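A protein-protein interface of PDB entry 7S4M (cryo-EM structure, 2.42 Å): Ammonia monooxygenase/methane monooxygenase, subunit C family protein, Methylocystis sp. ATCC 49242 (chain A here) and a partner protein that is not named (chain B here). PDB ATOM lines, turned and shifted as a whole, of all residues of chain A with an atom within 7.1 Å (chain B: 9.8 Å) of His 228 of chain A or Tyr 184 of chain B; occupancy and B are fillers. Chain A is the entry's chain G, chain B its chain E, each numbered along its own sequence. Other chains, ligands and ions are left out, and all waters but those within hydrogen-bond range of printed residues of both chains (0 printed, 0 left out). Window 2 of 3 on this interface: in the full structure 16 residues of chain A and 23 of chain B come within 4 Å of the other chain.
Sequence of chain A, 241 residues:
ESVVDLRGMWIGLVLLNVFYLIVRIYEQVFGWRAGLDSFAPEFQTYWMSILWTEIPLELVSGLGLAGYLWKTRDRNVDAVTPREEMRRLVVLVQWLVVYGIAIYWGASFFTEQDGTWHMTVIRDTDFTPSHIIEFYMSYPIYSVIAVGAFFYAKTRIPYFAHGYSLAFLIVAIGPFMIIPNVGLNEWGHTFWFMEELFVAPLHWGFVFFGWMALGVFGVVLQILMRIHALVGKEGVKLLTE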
ATOM      1  N   MET A  86       1.858 -20.616  -9.626  1.00  0.00           N
ATOM      2  CA  MET A  86       2.867 -20.052  -8.731  1.00  0.00           C
ATOM      3  C   MET A  86       4.077 -20.964  -8.610  1.00  0.00           C
ATOM      4  O   MET A  86       5.221 -20.495  -8.629  1.00  0.00           O
ATOM      5  CB  MET A  86       2.268 -19.783  -7.349  1.00  0.00           C
ATOM      6  CG  MET A  86       3.043 -18.768  -6.496  1.00  0.00           C
ATOM      7  SD  MET A  86       3.052 -17.001  -6.875  1.00  0.00           S
ATOM      8  CE  MET A  86       1.739 -16.838  -8.067  1.00  0.00           C
ATOM      9  N   LEU A  89       6.049 -20.622 -11.787  1.00  0.00           N
ATOM     10  CA  LEU A  89       6.752 -19.346 -11.821  1.00  0.00           C
ATOM     11  C   LEU A  89       7.983 -19.377 -10.929  1.00  0.00           C
ATOM     12  O   LEU A  89       9.039 -18.853 -11.295  1.00  0.00           O
ATOM     13  CB  LEU A  89       5.818 -18.215 -11.397  1.00  0.00           C
ATOM     14  CG  LEU A  89       4.795 -17.731 -12.421  1.00  0.00           C
ATOM     15  CD1 LEU A  89       3.821 -16.769 -11.774  1.00  0.00           C
ATOM     16  CD2 LEU A  89       5.485 -17.076 -13.597  1.00  0.00           C
ATOM     17  N   VAL A 220      11.738 -10.464 -16.046  1.00  0.00           N
ATOM     18  CA  VAL A 220      11.389 -10.334 -14.637  1.00  0.00           C
ATOM     19  C   VAL A 220      10.104  -9.535 -14.485  1.00  0.00           C
ATOM     20  O   VAL A 220       9.264  -9.842 -13.633  1.00  0.00           O
ATOM     21  CB  VAL A 220      12.554  -9.700 -13.858  1.00  0.00           C
ATOM     22  CG1 VAL A 220      12.090  -9.221 -12.500  1.00  0.00           C
ATOM     23  CG2 VAL A 220      13.682 -10.698 -13.712  1.00  0.00           C
ATOM     24  N   LEU A 221       9.919  -8.512 -15.318  1.00  0.00           N
ATOM     25  CA  LEU A 221       8.691  -7.729 -15.250  1.00  0.00           C
ATOM     26  C   LEU A 221       7.476  -8.567 -15.625  1.00  0.00           C
ATOM     27  O   LEU A 221       6.418  -8.441 -15.004  1.00  0.00           O
ATOM     28  CB  LEU A 221       8.799  -6.502 -16.149  1.00  0.00           C
ATOM     29  CG  LEU A 221       9.585  -5.340 -15.550  1.00  0.00           C
ATOM     30  CD1 LEU A 221       9.466  -4.119 -16.432  1.00  0.00           C
ATOM     31  CD2 LEU A 221       9.093  -5.037 -14.151  1.00  0.00           C
ATOM     32  N   GLN A 222       7.600  -9.422 -16.639  1.00  0.00           N
ATOM     33  CA  GLN A 222       6.488 -10.293 -17.005  1.00  0.00           C
ATOM     34  C   GLN A 222       6.197 -11.307 -15.907  1.00  0.00           C
ATOM     35  O   GLN A 222       5.031 -11.601 -15.611  1.00  0.00           O
ATOM     36  CB  GLN A 222       6.787 -11.000 -18.324  1.00  0.00           C
ATOM     37  CG  GLN A 222       6.826 -10.069 -19.517  1.00  0.00           C
ATOM     38  CD  GLN A 222       7.355 -10.740 -20.763  1.00  0.00           C
ATOM     39  OE1 GLN A 222       8.235 -11.595 -20.693  1.00  0.00           O
ATOM     40  NE2 GLN A 222       6.824 -10.353 -21.914  1.00  0.00           N
ATOM     41  N   ILE A 223       7.246 -11.848 -15.287  1.00  0.00           N
ATOM     42  CA  ILE A 223       7.050 -12.768 -14.172  1.00  0.00           C
ATOM     43  C   ILE A 223       6.331 -12.066 -13.031  1.00  0.00           C
ATOM     44  O   ILE A 223       5.431 -12.630 -12.399  1.00  0.00           O
ATOM     45  CB  ILE A 223       8.400 -13.348 -13.718  1.00  0.00           C
ATOM     46  CG1 ILE A 223       8.954 -14.285 -14.786  1.00  0.00           C
ATOM     47  CG2 ILE A 223       8.250 -14.075 -12.399  1.00  0.00           C
ATOM     48  CD1 ILE A 223      10.255 -14.927 -14.399  1.00  0.00           C
ATOM     49  N   LEU A 224       6.715 -10.822 -12.750  1.00  0.00           N
ATOM     50  CA  LEU A 224       6.060 -10.065 -11.692  1.00  0.00           C
ATOM     51  C   LEU A 224       4.619  -9.741 -12.054  1.00  0.00           C
ATOM     52  O   LEU A 224       3.753  -9.705 -11.178  1.00  0.00           O
ATOM     53  CB  LEU A 224       6.843  -8.790 -11.407  1.00  0.00           C
ATOM     54  CG  LEU A 224       8.112  -9.005 -10.589  1.00  0.00           C
ATOM     55  CD1 LEU A 224       8.938  -7.744 -10.567  1.00  0.00           C
ATOM     56  CD2 LEU A 224       7.762  -9.441  -9.184  1.00  0.00           C
ATOM     57  N   MET A 225       4.346  -9.485 -13.333  1.00  0.00           N
ATOM     58  CA  MET A 225       2.967  -9.295 -13.769  1.00  0.00           C
ATOM     59  C   MET A 225       2.142 -10.539 -13.485  1.00  0.00           C
ATOM     60  O   MET A 225       1.025 -10.457 -12.963  1.00  0.00           O
ATOM     61  CB  MET A 225       2.928  -8.962 -15.259  1.00  0.00           C
ATOM     62  CG  MET A 225       2.791  -7.487 -15.576  1.00  0.00           C
ATOM     63  SD  MET A 225       3.058  -7.122 -17.322  1.00  0.00           S
ATOM     64  CE  MET A 225       2.590  -8.677 -18.074  1.00  0.00           C
ATOM     65  N   ARG A 226       2.690 -11.708 -13.814  1.00  0.00           N
ATOM     66  CA  ARG A 226       1.979 -12.954 -13.551  1.00  0.00           C
ATOM     67  C   ARG A 226       1.766 -13.163 -12.058  1.00  0.00           C
ATOM     68  O   ARG A 226       0.690 -13.594 -11.630  1.00  0.00           O
ATOM     69  CB  ARG A 226       2.741 -14.129 -14.156  1.00  0.00           C
ATOM     70  CG  ARG A 226       2.429 -14.379 -15.618  1.00  0.00           C
ATOM     71  CD  ARG A 226       0.989 -14.032 -15.941  1.00  0.00           C
ATOM     72  NE  ARG A 226       0.063 -15.002 -15.372  1.00  0.00           N
ATOM     73  CZ  ARG A 226      -1.212 -14.755 -15.113  1.00  0.00           C
ATOM     74  NH1 ARG A 226      -1.747 -13.569 -15.350  1.00  0.00           N
ATOM     75  NH2 ARG A 226      -1.969 -15.720 -14.601  1.00  0.00           N
ATOM     76  N   ILE A 227       2.782 -12.863 -11.249  1.00  0.00           N
ATOM     77  CA  ILE A 227       2.669 -13.055  -9.806  1.00  0.00           C
ATOM     78  C   ILE A 227       1.613 -12.123  -9.228  1.00  0.00           C
ATOM     79  O   ILE A 227       0.732 -12.542  -8.470  1.00  0.00           O
ATOM     80  CB  ILE A 227       4.033 -12.841  -9.129  1.00  0.00           C
ATOM     81  CG1 ILE A 227       4.920 -14.067  -9.321  1.00  0.00           C
ATOM     82  CG2 ILE A 227       3.853 -12.552  -7.652  1.00  0.00           C
ATOM     83  CD1 ILE A 227       6.318 -13.882  -8.788  1.00  0.00           C
ATOM     84  N   HIS A 228       1.686 -10.842  -9.588  1.00  0.00           N
ATOM     85  CA  HIS A 228       0.754  -9.853  -9.065  1.00  0.00           C
ATOM     86  C   HIS A 228      -0.668 -10.119  -9.531  1.00  0.00           C
ATOM     87  O   HIS A 228      -1.621  -9.830  -8.802  1.00  0.00           O
ATOM     88  CB  HIS A 228       1.212  -8.457  -9.481  1.00  0.00           C
ATOM     89  CG  HIS A 228       0.122  -7.435  -9.484  1.00  0.00           C
ATOM     90  ND1 HIS A 228      -0.555  -7.067  -8.343  1.00  0.00           N
ATOM     91  CD2 HIS A 228      -0.400  -6.693 -10.488  1.00  0.00           C
ATOM     92  CE1 HIS A 228      -1.454  -6.147  -8.645  1.00  0.00           C
ATOM     93  NE2 HIS A 228      -1.379  -5.902  -9.940  1.00  0.00           N
ATOM     94  N   ALA A 229      -0.833 -10.665 -10.735  1.00  0.00           N
ATOM     95  CA  ALA A 229      -2.167 -11.017 -11.198  1.00  0.00           C
ATOM     96  C   ALA A 229      -2.719 -12.232 -10.468  1.00  0.00           C
ATOM     97  O   ALA A 229      -3.933 -12.325 -10.263  1.00  0.00           O
ATOM     98  CB  ALA A 229      -2.151 -11.274 -12.705  1.00  0.00           C
ATOM     99  N   LEU A 230      -1.855 -13.166 -10.071  1.00  0.00           N
ATOM    100  CA  LEU A 230      -2.344 -14.386  -9.438  1.00  0.00           C
ATOM    101  C   LEU A 230      -2.792 -14.140  -8.005  1.00  0.00           C
ATOM    102  O   LEU A 230      -3.830 -14.660  -7.581  1.00  0.00           O
ATOM    103  CB  LEU A 230      -1.278 -15.470  -9.479  1.00  0.00           C
ATOM    104  CG  LEU A 230      -1.225 -16.225 -10.799  1.00  0.00           C
ATOM    105  CD1 LEU A 230      -0.537 -17.535 -10.573  1.00  0.00           C
ATOM    106  CD2 LEU A 230      -2.617 -16.441 -11.360  1.00  0.00           C
ATOM    107  N   VAL A 231      -2.022 -13.373  -7.237  1.00  0.00           N
ATOM    108  CA  VAL A 231      -2.438 -13.059  -5.876  1.00  0.00           C
ATOM    109  C   VAL A 231      -3.732 -12.260  -5.948  1.00  0.00           C
ATOM    110  O   VAL A 231      -3.833 -11.274  -6.687  1.00  0.00           O
ATOM    111  CB  VAL A 231      -1.340 -12.305  -5.117  1.00  0.00           C
ATOM    112  CG1 VAL A 231      -0.178 -13.234  -4.820  1.00  0.00           C
ATOM    113  CG2 VAL A 231      -0.859 -11.107  -5.910  1.00  0.00           C
ATOM    114  N   GLY A 232      -4.737 -12.702  -5.201  1.00  0.00           N
ATOM    115  CA  GLY A 232      -6.062 -12.126  -5.312  1.00  0.00           C
ATOM    116  C   GLY A 232      -6.144 -10.692  -4.842  1.00  0.00           C
ATOM    117  O   GLY A 232      -5.130 -10.087  -4.482  1.00  0.00           O
ATOM    118  N   LYS A 233      -7.358 -10.137  -4.845  1.00  0.00           N
ATOM    119  CA  LYS A 233      -7.546  -8.772  -4.370  1.00  0.00           C
ATOM    120  C   LYS A 233      -7.103  -8.622  -2.922  1.00  0.00           C
ATOM    121  O   LYS A 233      -6.638  -7.550  -2.523  1.00  0.00           O
ATOM    122  CB  LYS A 233      -9.014  -8.364  -4.523  1.00  0.00           C
ATOM    123  CG  LYS A 233      -9.547  -8.085  -5.959  1.00  0.00           C
ATOM    124  CD  LYS A 233      -8.622  -7.446  -7.034  1.00  0.00           C
ATOM    125  CE  LYS A 233      -7.621  -6.397  -6.545  1.00  0.00           C
ATOM    126  NZ  LYS A 233      -8.268  -5.403  -5.647  1.00  0.00           N
ATOM    127  N   GLY A 235      -4.615 -10.419  -1.624  1.00  0.00           N
ATOM    128  CA  GLY A 235      -3.167 -10.521  -1.616  1.00  0.00           C
ATOM    129  C   GLY A 235      -2.482  -9.209  -1.947  1.00  0.00           C
ATOM    130  O   GLY A 235      -1.515  -8.823  -1.286  1.00  0.00           O
ATOM    131  N   VAL A 236      -2.975  -8.505  -2.967  1.00  0.00           N
ATOM    132  CA  VAL A 236      -2.305  -7.291  -3.426  1.00  0.00           C
ATOM    133  C   VAL A 236      -2.383  -6.200  -2.367  1.00  0.00           C
ATOM    134  O   VAL A 236      -1.373  -5.583  -2.011  1.00  0.00           O
ATOM    135  CB  VAL A 236      -2.901  -6.824  -4.767  1.00  0.00           C
ATOM    136  CG1 VAL A 236      -4.405  -6.986  -4.769  1.00  0.00           C
ATOM    137  CG2 VAL A 236      -2.536  -5.377  -5.030  1.00  0.00           C
ATOM    138  N   LYS B 178      11.877  -1.706   1.650  1.00  0.00           N
ATOM    139  CA  LYS B 178      10.824  -1.940   0.673  1.00  0.00           C
ATOM    140  C   LYS B 178      11.167  -3.193  -0.115  1.00  0.00           C
ATOM    141  O   LYS B 178      12.237  -3.273  -0.723  1.00  0.00           O
ATOM    142  CB  LYS B 178      10.672  -0.745  -0.270  1.00  0.00           C
ATOM    143  CG  LYS B 178      10.027   0.468   0.368  1.00  0.00           C
ATOM    144  CD  LYS B 178      11.065   1.397   0.961  1.00  0.00           C
ATOM    145  CE  LYS B 178      10.409   2.510   1.756  1.00  0.00           C
ATOM    146  NZ  LYS B 178      11.402   3.302   2.528  1.00  0.00           N
ATOM    147  N   GLY B 179      10.262  -4.164  -0.107  1.00  0.00           N
ATOM    148  CA  GLY B 179      10.486  -5.396  -0.829  1.00  0.00           C
ATOM    149  C   GLY B 179      10.434  -5.179  -2.327  1.00  0.00           C
ATOM    150  O   GLY B 179       9.992  -4.148  -2.832  1.00  0.00           O
ATOM    151  N   ILE B 180      10.905  -6.184  -3.060  1.00  0.00           N
ATOM    152  CA  ILE B 180      10.914  -6.106  -4.516  1.00  0.00           C
ATOM    153  C   ILE B 180       9.506  -6.349  -5.035  1.00  0.00           C
ATOM    154  O   ILE B 180       8.949  -5.516  -5.758  1.00  0.00           O
ATOM    155  CB  ILE B 180      11.912  -7.102  -5.130  1.00  0.00           C
ATOM    156  CG1 ILE B 180      13.344  -6.652  -4.855  1.00  0.00           C
ATOM    157  CG2 ILE B 180      11.675  -7.234  -6.620  1.00  0.00           C
ATOM    158  CD1 ILE B 180      14.388  -7.480  -5.561  1.00  0.00           C
ATOM    159  N   ILE B 181       8.920  -7.491  -4.670  1.00  0.00           N
ATOM    160  CA  ILE B 181       7.548  -7.781  -5.079  1.00  0.00           C
ATOM    161  C   ILE B 181       6.587  -6.770  -4.472  1.00  0.00           C
ATOM    162  O   ILE B 181       5.674  -6.277  -5.144  1.00  0.00           O
ATOM    163  CB  ILE B 181       7.165  -9.219  -4.691  1.00  0.00           C
ATOM    164  CG1 ILE B 181       7.899 -10.222  -5.577  1.00  0.00           C
ATOM    165  CG2 ILE B 181       5.668  -9.419  -4.798  1.00  0.00           C
ATOM    166  CD1 ILE B 181       7.729 -11.646  -5.133  1.00  0.00           C
ATOM    167  N   THR B 182       6.776  -6.449  -3.193  1.00  0.00           N
ATOM    168  CA  THR B 182       5.868  -5.530  -2.516  1.00  0.00           C
ATOM    169  C   THR B 182       5.866  -4.167  -3.191  1.00  0.00           C
ATOM    170  O   THR B 182       4.804  -3.621  -3.514  1.00  0.00           O
ATOM    171  CB  THR B 182       6.262  -5.401  -1.049  1.00  0.00           C
ATOM    172  OG1 THR B 182       6.080  -6.659  -0.392  1.00  0.00           O
ATOM    173  CG2 THR B 182       5.409  -4.355  -0.366  1.00  0.00           C
ATOM    174  N   SER B 183       7.052  -3.604  -3.428  1.00  0.00           N
ATOM    175  CA  SER B 183       7.123  -2.288  -4.050  1.00  0.00           C
ATOM    176  C   SER B 183       6.669  -2.327  -5.501  1.00  0.00           C
ATOM    177  O   SER B 183       6.072  -1.360  -5.980  1.00  0.00           O
ATOM    178  CB  SER B 183       8.539  -1.727  -3.955  1.00  0.00           C
ATOM    179  OG  SER B 183       9.426  -2.458  -4.778  1.00  0.00           O
ATOM    180  N   TYR B 184       6.941  -3.419  -6.216  1.00  0.00           N
ATOM    181  CA  TYR B 184       6.451  -3.528  -7.585  1.00  0.00           C
ATOM    182  C   TYR B 184       4.930  -3.505  -7.619  1.00  0.00           C
ATOM    183  O   TYR B 184       4.327  -2.806  -8.438  1.00  0.00           O
ATOM    184  CB  TYR B 184       6.960  -4.804  -8.244  1.00  0.00           C
ATOM    185  CG  TYR B 184       6.162  -5.161  -9.471  1.00  0.00           C
ATOM    186  CD1 TYR B 184       6.375  -4.503 -10.670  1.00  0.00           C
ATOM    187  CD2 TYR B 184       5.178  -6.135  -9.425  1.00  0.00           C
ATOM    188  CE1 TYR B 184       5.642  -4.813 -11.791  1.00  0.00           C
ATOM    189  CE2 TYR B 184       4.437  -6.448 -10.539  1.00  0.00           C
ATOM    190  CZ  TYR B 184       4.677  -5.787 -11.719  1.00  0.00           C
ATOM    191  OH  TYR B 184       3.943  -6.100 -12.834  1.00  0.00           O
ATOM    192  N   ILE B 185       4.296  -4.288  -6.746  1.00  0.00           N
ATOM    193  CA  ILE B 185       2.839  -4.307  -6.686  1.00  0.00           C
ATOM    194  C   ILE B 185       2.314  -2.933  -6.307  1.00  0.00           C
ATOM    195  O   ILE B 185       1.350  -2.431  -6.898  1.00  0.00           O
ATOM    196  CB  ILE B 185       2.366  -5.390  -5.699  1.00  0.00           C
ATOM    197  CG1 ILE B 185       2.286  -6.745  -6.397  1.00  0.00           C
ATOM    198  CG2 ILE B 185       1.022  -5.023  -5.099  1.00  0.00           C
ATOM    199  CD1 ILE B 185       2.204  -7.907  -5.445  1.00  0.00           C
ATOM    200  N   ARG B 186       2.957  -2.296  -5.329  1.00  0.00           N
ATOM    201  CA  ARG B 186       2.543  -0.968  -4.902  1.00  0.00           C
ATOM    202  C   ARG B 186       2.604   0.025  -6.056  1.00  0.00           C
ATOM    203  O   ARG B 186       1.661   0.794  -6.275  1.00  0.00           O
ATOM    204  CB  ARG B 186       3.428  -0.519  -3.743  1.00  0.00           C
ATOM    205  CG  ARG B 186       3.055   0.803  -3.135  1.00  0.00           C
ATOM    206  CD  ARG B 186       3.545   0.904  -1.708  1.00  0.00           C
ATOM    207  NE  ARG B 186       3.527  -0.381  -1.021  1.00  0.00           N
ATOM    208  CZ  ARG B 186       3.891  -0.552   0.241  1.00  0.00           C
ATOM    209  NH1 ARG B 186       4.329   0.456   0.976  1.00  0.00           N
ATOM    210  NH2 ARG B 186       3.813  -1.763   0.781  1.00  0.00           N
ATOM    211  N   VAL B 187       3.696   0.007  -6.819  1.00  0.00           N
ATOM    212  CA  VAL B 187       3.838   0.916  -7.951  1.00  0.00           C
ATOM    213  C   VAL B 187       2.800   0.611  -9.020  1.00  0.00           C
ATOM    214  O   VAL B 187       2.175   1.521  -9.576  1.00  0.00           O
ATOM    215  CB  VAL B 187       5.268   0.842  -8.514  1.00  0.00           C
ATOM    216  CG1 VAL B 187       5.318   1.414  -9.916  1.00  0.00           C
ATOM    217  CG2 VAL B 187       6.230   1.585  -7.608  1.00  0.00           C
ATOM    218  N   ALA B 188       2.595  -0.671  -9.324  1.00  0.00           N
ATOM    219  CA  ALA B 188       1.630  -1.049 -10.347  1.00  0.00           C
ATOM    220  C   ALA B 188       0.204  -0.695  -9.957  1.00  0.00           C
ATOM    221  O   ALA B 188      -0.637  -0.509 -10.842  1.00  0.00           O
ATOM    222  CB  ALA B 188       1.732  -2.546 -10.636  1.00  0.00           C
ATOM    223  N   GLU B 189      -0.075  -0.637  -8.654  1.00  0.00           N
ATOM    224  CA  GLU B 189      -1.451  -0.318  -8.186  1.00  0.00           C
ATOM    225  C   GLU B 189      -1.642   1.201  -8.171  1.00  0.00           C
ATOM    226  O   GLU B 189      -2.513   1.676  -7.418  1.00  0.00           O
ATOM    227  CB  GLU B 189      -1.707  -0.944  -6.815  1.00  0.00           C
ATOM    228  CG  GLU B 189      -2.042  -2.414  -6.906  1.00  0.00           C
ATOM    229  CD  GLU B 189      -3.450  -2.713  -7.391  1.00  0.00           C
ATOM    230  OE1 GLU B 189      -4.396  -2.506  -6.608  1.00  0.00           O
ATOM    231  OE2 GLU B 189      -3.594  -3.158  -8.546  1.00  0.00           O
ATOM    232  N   GLY B 190      -0.856   1.930  -8.970  1.00  0.00           N
ATOM    233  CA  GLY B 190      -1.004   3.393  -9.064  1.00  0.00           C
ATOM    234  C   GLY B 190      -0.253   4.129  -7.970  1.00  0.00           C
ATOM    235  O   GLY B 190       0.312   5.197  -8.276  1.00  0.00           O
ATOM    236  N   LYS B 191      -0.243   3.576  -6.753  1.00  0.00           N
ATOM    237  CA  LYS B 191       0.381   4.262  -5.592  1.00  0.00           C
ATOM    238  C   LYS B 191       1.899   4.062  -5.598  1.00  0.00           C
ATOM    239  O   LYS B 191       2.410   3.397  -4.679  1.00  0.00           O
ATOM    240  CB  LYS B 191      -0.245   3.747  -4.291  1.00  0.00           C
ATOM    241  CG  LYS B 191      -0.776   2.320  -4.338  1.00  0.00           C
ATOM    242  CD  LYS B 191      -0.425   1.511  -3.110  1.00  0.00           C
ATOM    243  CE  LYS B 191      -0.566   0.019  -3.322  1.00  0.00           C
ATOM    244  NZ  LYS B 191      -1.988  -0.391  -3.399  1.00  0.00           N
ATOM    245  N   ALA B 192       2.599   4.633  -6.580  1.00  0.00           N
ATOM    246  CA  ALA B 192       4.079   4.571  -6.587  1.00  0.00           C
ATOM    247  C   ALA B 192       4.615   5.790  -5.828  1.00  0.00           C
ATOM    248  O   ALA B 192       5.659   6.334  -6.239  1.00  0.00           O
ATOM    249  CB  ALA B 192       4.576   4.520  -8.007  1.00  0.00           C
ATOM    250  N   ASP B 193       3.924   6.198  -4.759  1.00  0.00           N
ATOM    251  CA  ASP B 193       4.323   7.398  -3.976  1.00  0.00           C
ATOM    252  C   ASP B 193       4.550   6.992  -2.519  1.00  0.00           C
ATOM    253  O   ASP B 193       5.394   7.625  -1.863  1.00  0.00           O
ATOM    254  CB  ASP B 193       3.273   8.504  -4.079  1.00  0.00           C
ATOM    255  CG  ASP B 193       2.732   8.699  -5.483  1.00  0.00           C
ATOM    256  OD1 ASP B 193       3.404   9.384  -6.276  1.00  0.00           O
ATOM    257  OD2 ASP B 193       1.646   8.158  -5.774  1.00  0.00           O
ATOM    258  N   ASP B 194       3.816   5.988  -2.030  1.00  0.00           N
ATOM    259  CA  ASP B 194       4.052   5.484  -0.648  1.00  0.00           C
ATOM    260  C   ASP B 194       5.160   4.419  -0.680  1.00  0.00           C
ATOM    261  O   ASP B 194       5.491   3.896   0.400  1.00  0.00           O
ATOM    262  CB  ASP B 194       2.749   5.043   0.030  1.00  0.00           C
ATOM    263  CG  ASP B 194       2.134   3.768  -0.519  1.00  0.00           C
ATOM    264  OD1 ASP B 194       1.764   3.757  -1.708  1.00  0.00           O
ATOM    265  OD2 ASP B 194       2.007   2.804   0.259  1.00  0.00           O
ATOM    266  N   VAL B 195       5.702   4.109  -1.864  1.00  0.00           N
ATOM    267  CA  VAL B 195       6.868   3.178  -1.949  1.00  0.00           C
ATOM    268  C   VAL B 195       8.126   4.009  -1.681  1.00  0.00           C
ATOM    269  O   VAL B 195       8.994   3.521  -0.937  1.00  0.00           O
ATOM    270  CB  VAL B 195       6.924   2.444  -3.302  1.00  0.00           C
ATOM    271  CG1 VAL B 195       6.576   3.357  -4.465  1.00  0.00           C
ATOM    272  CG2 VAL B 195       8.265   1.765  -3.529  1.00  0.00           C
ATOM    273  N   ILE B 196       8.212   5.220  -2.247  1.00  0.00           N
ATOM    274  CA  ILE B 196       9.359   6.133  -1.942  1.00  0.00           C
ATOM    275  C   ILE B 196       8.810   7.548  -1.720  1.00  0.00           C
ATOM    276  O   ILE B 196       8.209   8.105  -2.662  1.00  0.00           O
ATOM    277  CB  ILE B 196      10.465   6.060  -3.017  1.00  0.00           C
ATOM    278  CG1 ILE B 196      11.545   5.054  -2.614  1.00  0.00           C
ATOM    279  CG2 ILE B 196      11.065   7.426  -3.315  1.00  0.00           C
ATOM    280  CD1 ILE B 196      12.692   5.664  -1.850  1.00  0.00           C
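CG1 of Ile 181 of chain B touches CD2 of Leu 224 of chain A, 3.7 Å away.
Tyr 184 of chain B touches Leu 224 of chain A.
CB of His 228 of chain A touches CE2 of Tyr 184 of chain B, at 3.9 Å.
Ile 185 of chain B touches His 228 of chain A.
Glu 189 of chain B touches His 228 of chain A (OE2 to CE1, 3.7 Å).
CG2 of Ile 185 of chain B touches CG2 of Val 236 of chain A, at 3.6 Å.
CG2 of Val 236 of chain A touches CG of Glu 189 of chain B, at 3.5 Å.
Printed residues of chain B that touch a printed residue of chain A: Ile 181, Tyr 184, Ile 185 and Glu 189.
Hydrophobic or aromatic side chains of chain B that line the printed part of chain A: Ile 181, Tyr 184 and Ile 185.
Hydrophobic or aromatic side chains of chain A within 4 Å of the printed part of chain B: Leu 224, Met 225, His 228 and Val 236.
Of chain B, only Tyr 184 (3.9 Å), Ile 185 (3.5 Å) and Glu 189 (3.7 Å) come within 4 Å of His 228 of chain A.
Tyr 184 of chain B touches just these residues of chain A: Leu 224, Met 225 and His 228.
Leu 224 of chain A touches just these residues of chain B: Ile 181 and Tyr 184.
No residue of chain B comes within 4 Å of Ile 227 of chain A.
No residue of chain B comes within 4 Å of Val 231 of chain A.
Printed residues of chain B within 4 Å of Val 236 of chain A: Ile 185 (3.6 Å) and Glu 189 (3.5 Å).
Of the printed residues of chain A, Ile 185 of chain B touches His 228 (3.5 Å) and Val 236 (3.6 Å).
Gly 235 of chain A touches none of the printed residues of chain B.
The nearest printed residue of chain B that does not touch Met 225 of chain A is Ala 188 of chain B (7.1 Å).
The side-chain hydroxyl of Tyr 184 of chain B lies close to the backbone NH of Met 225 of chain A, 3.4 Å away.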
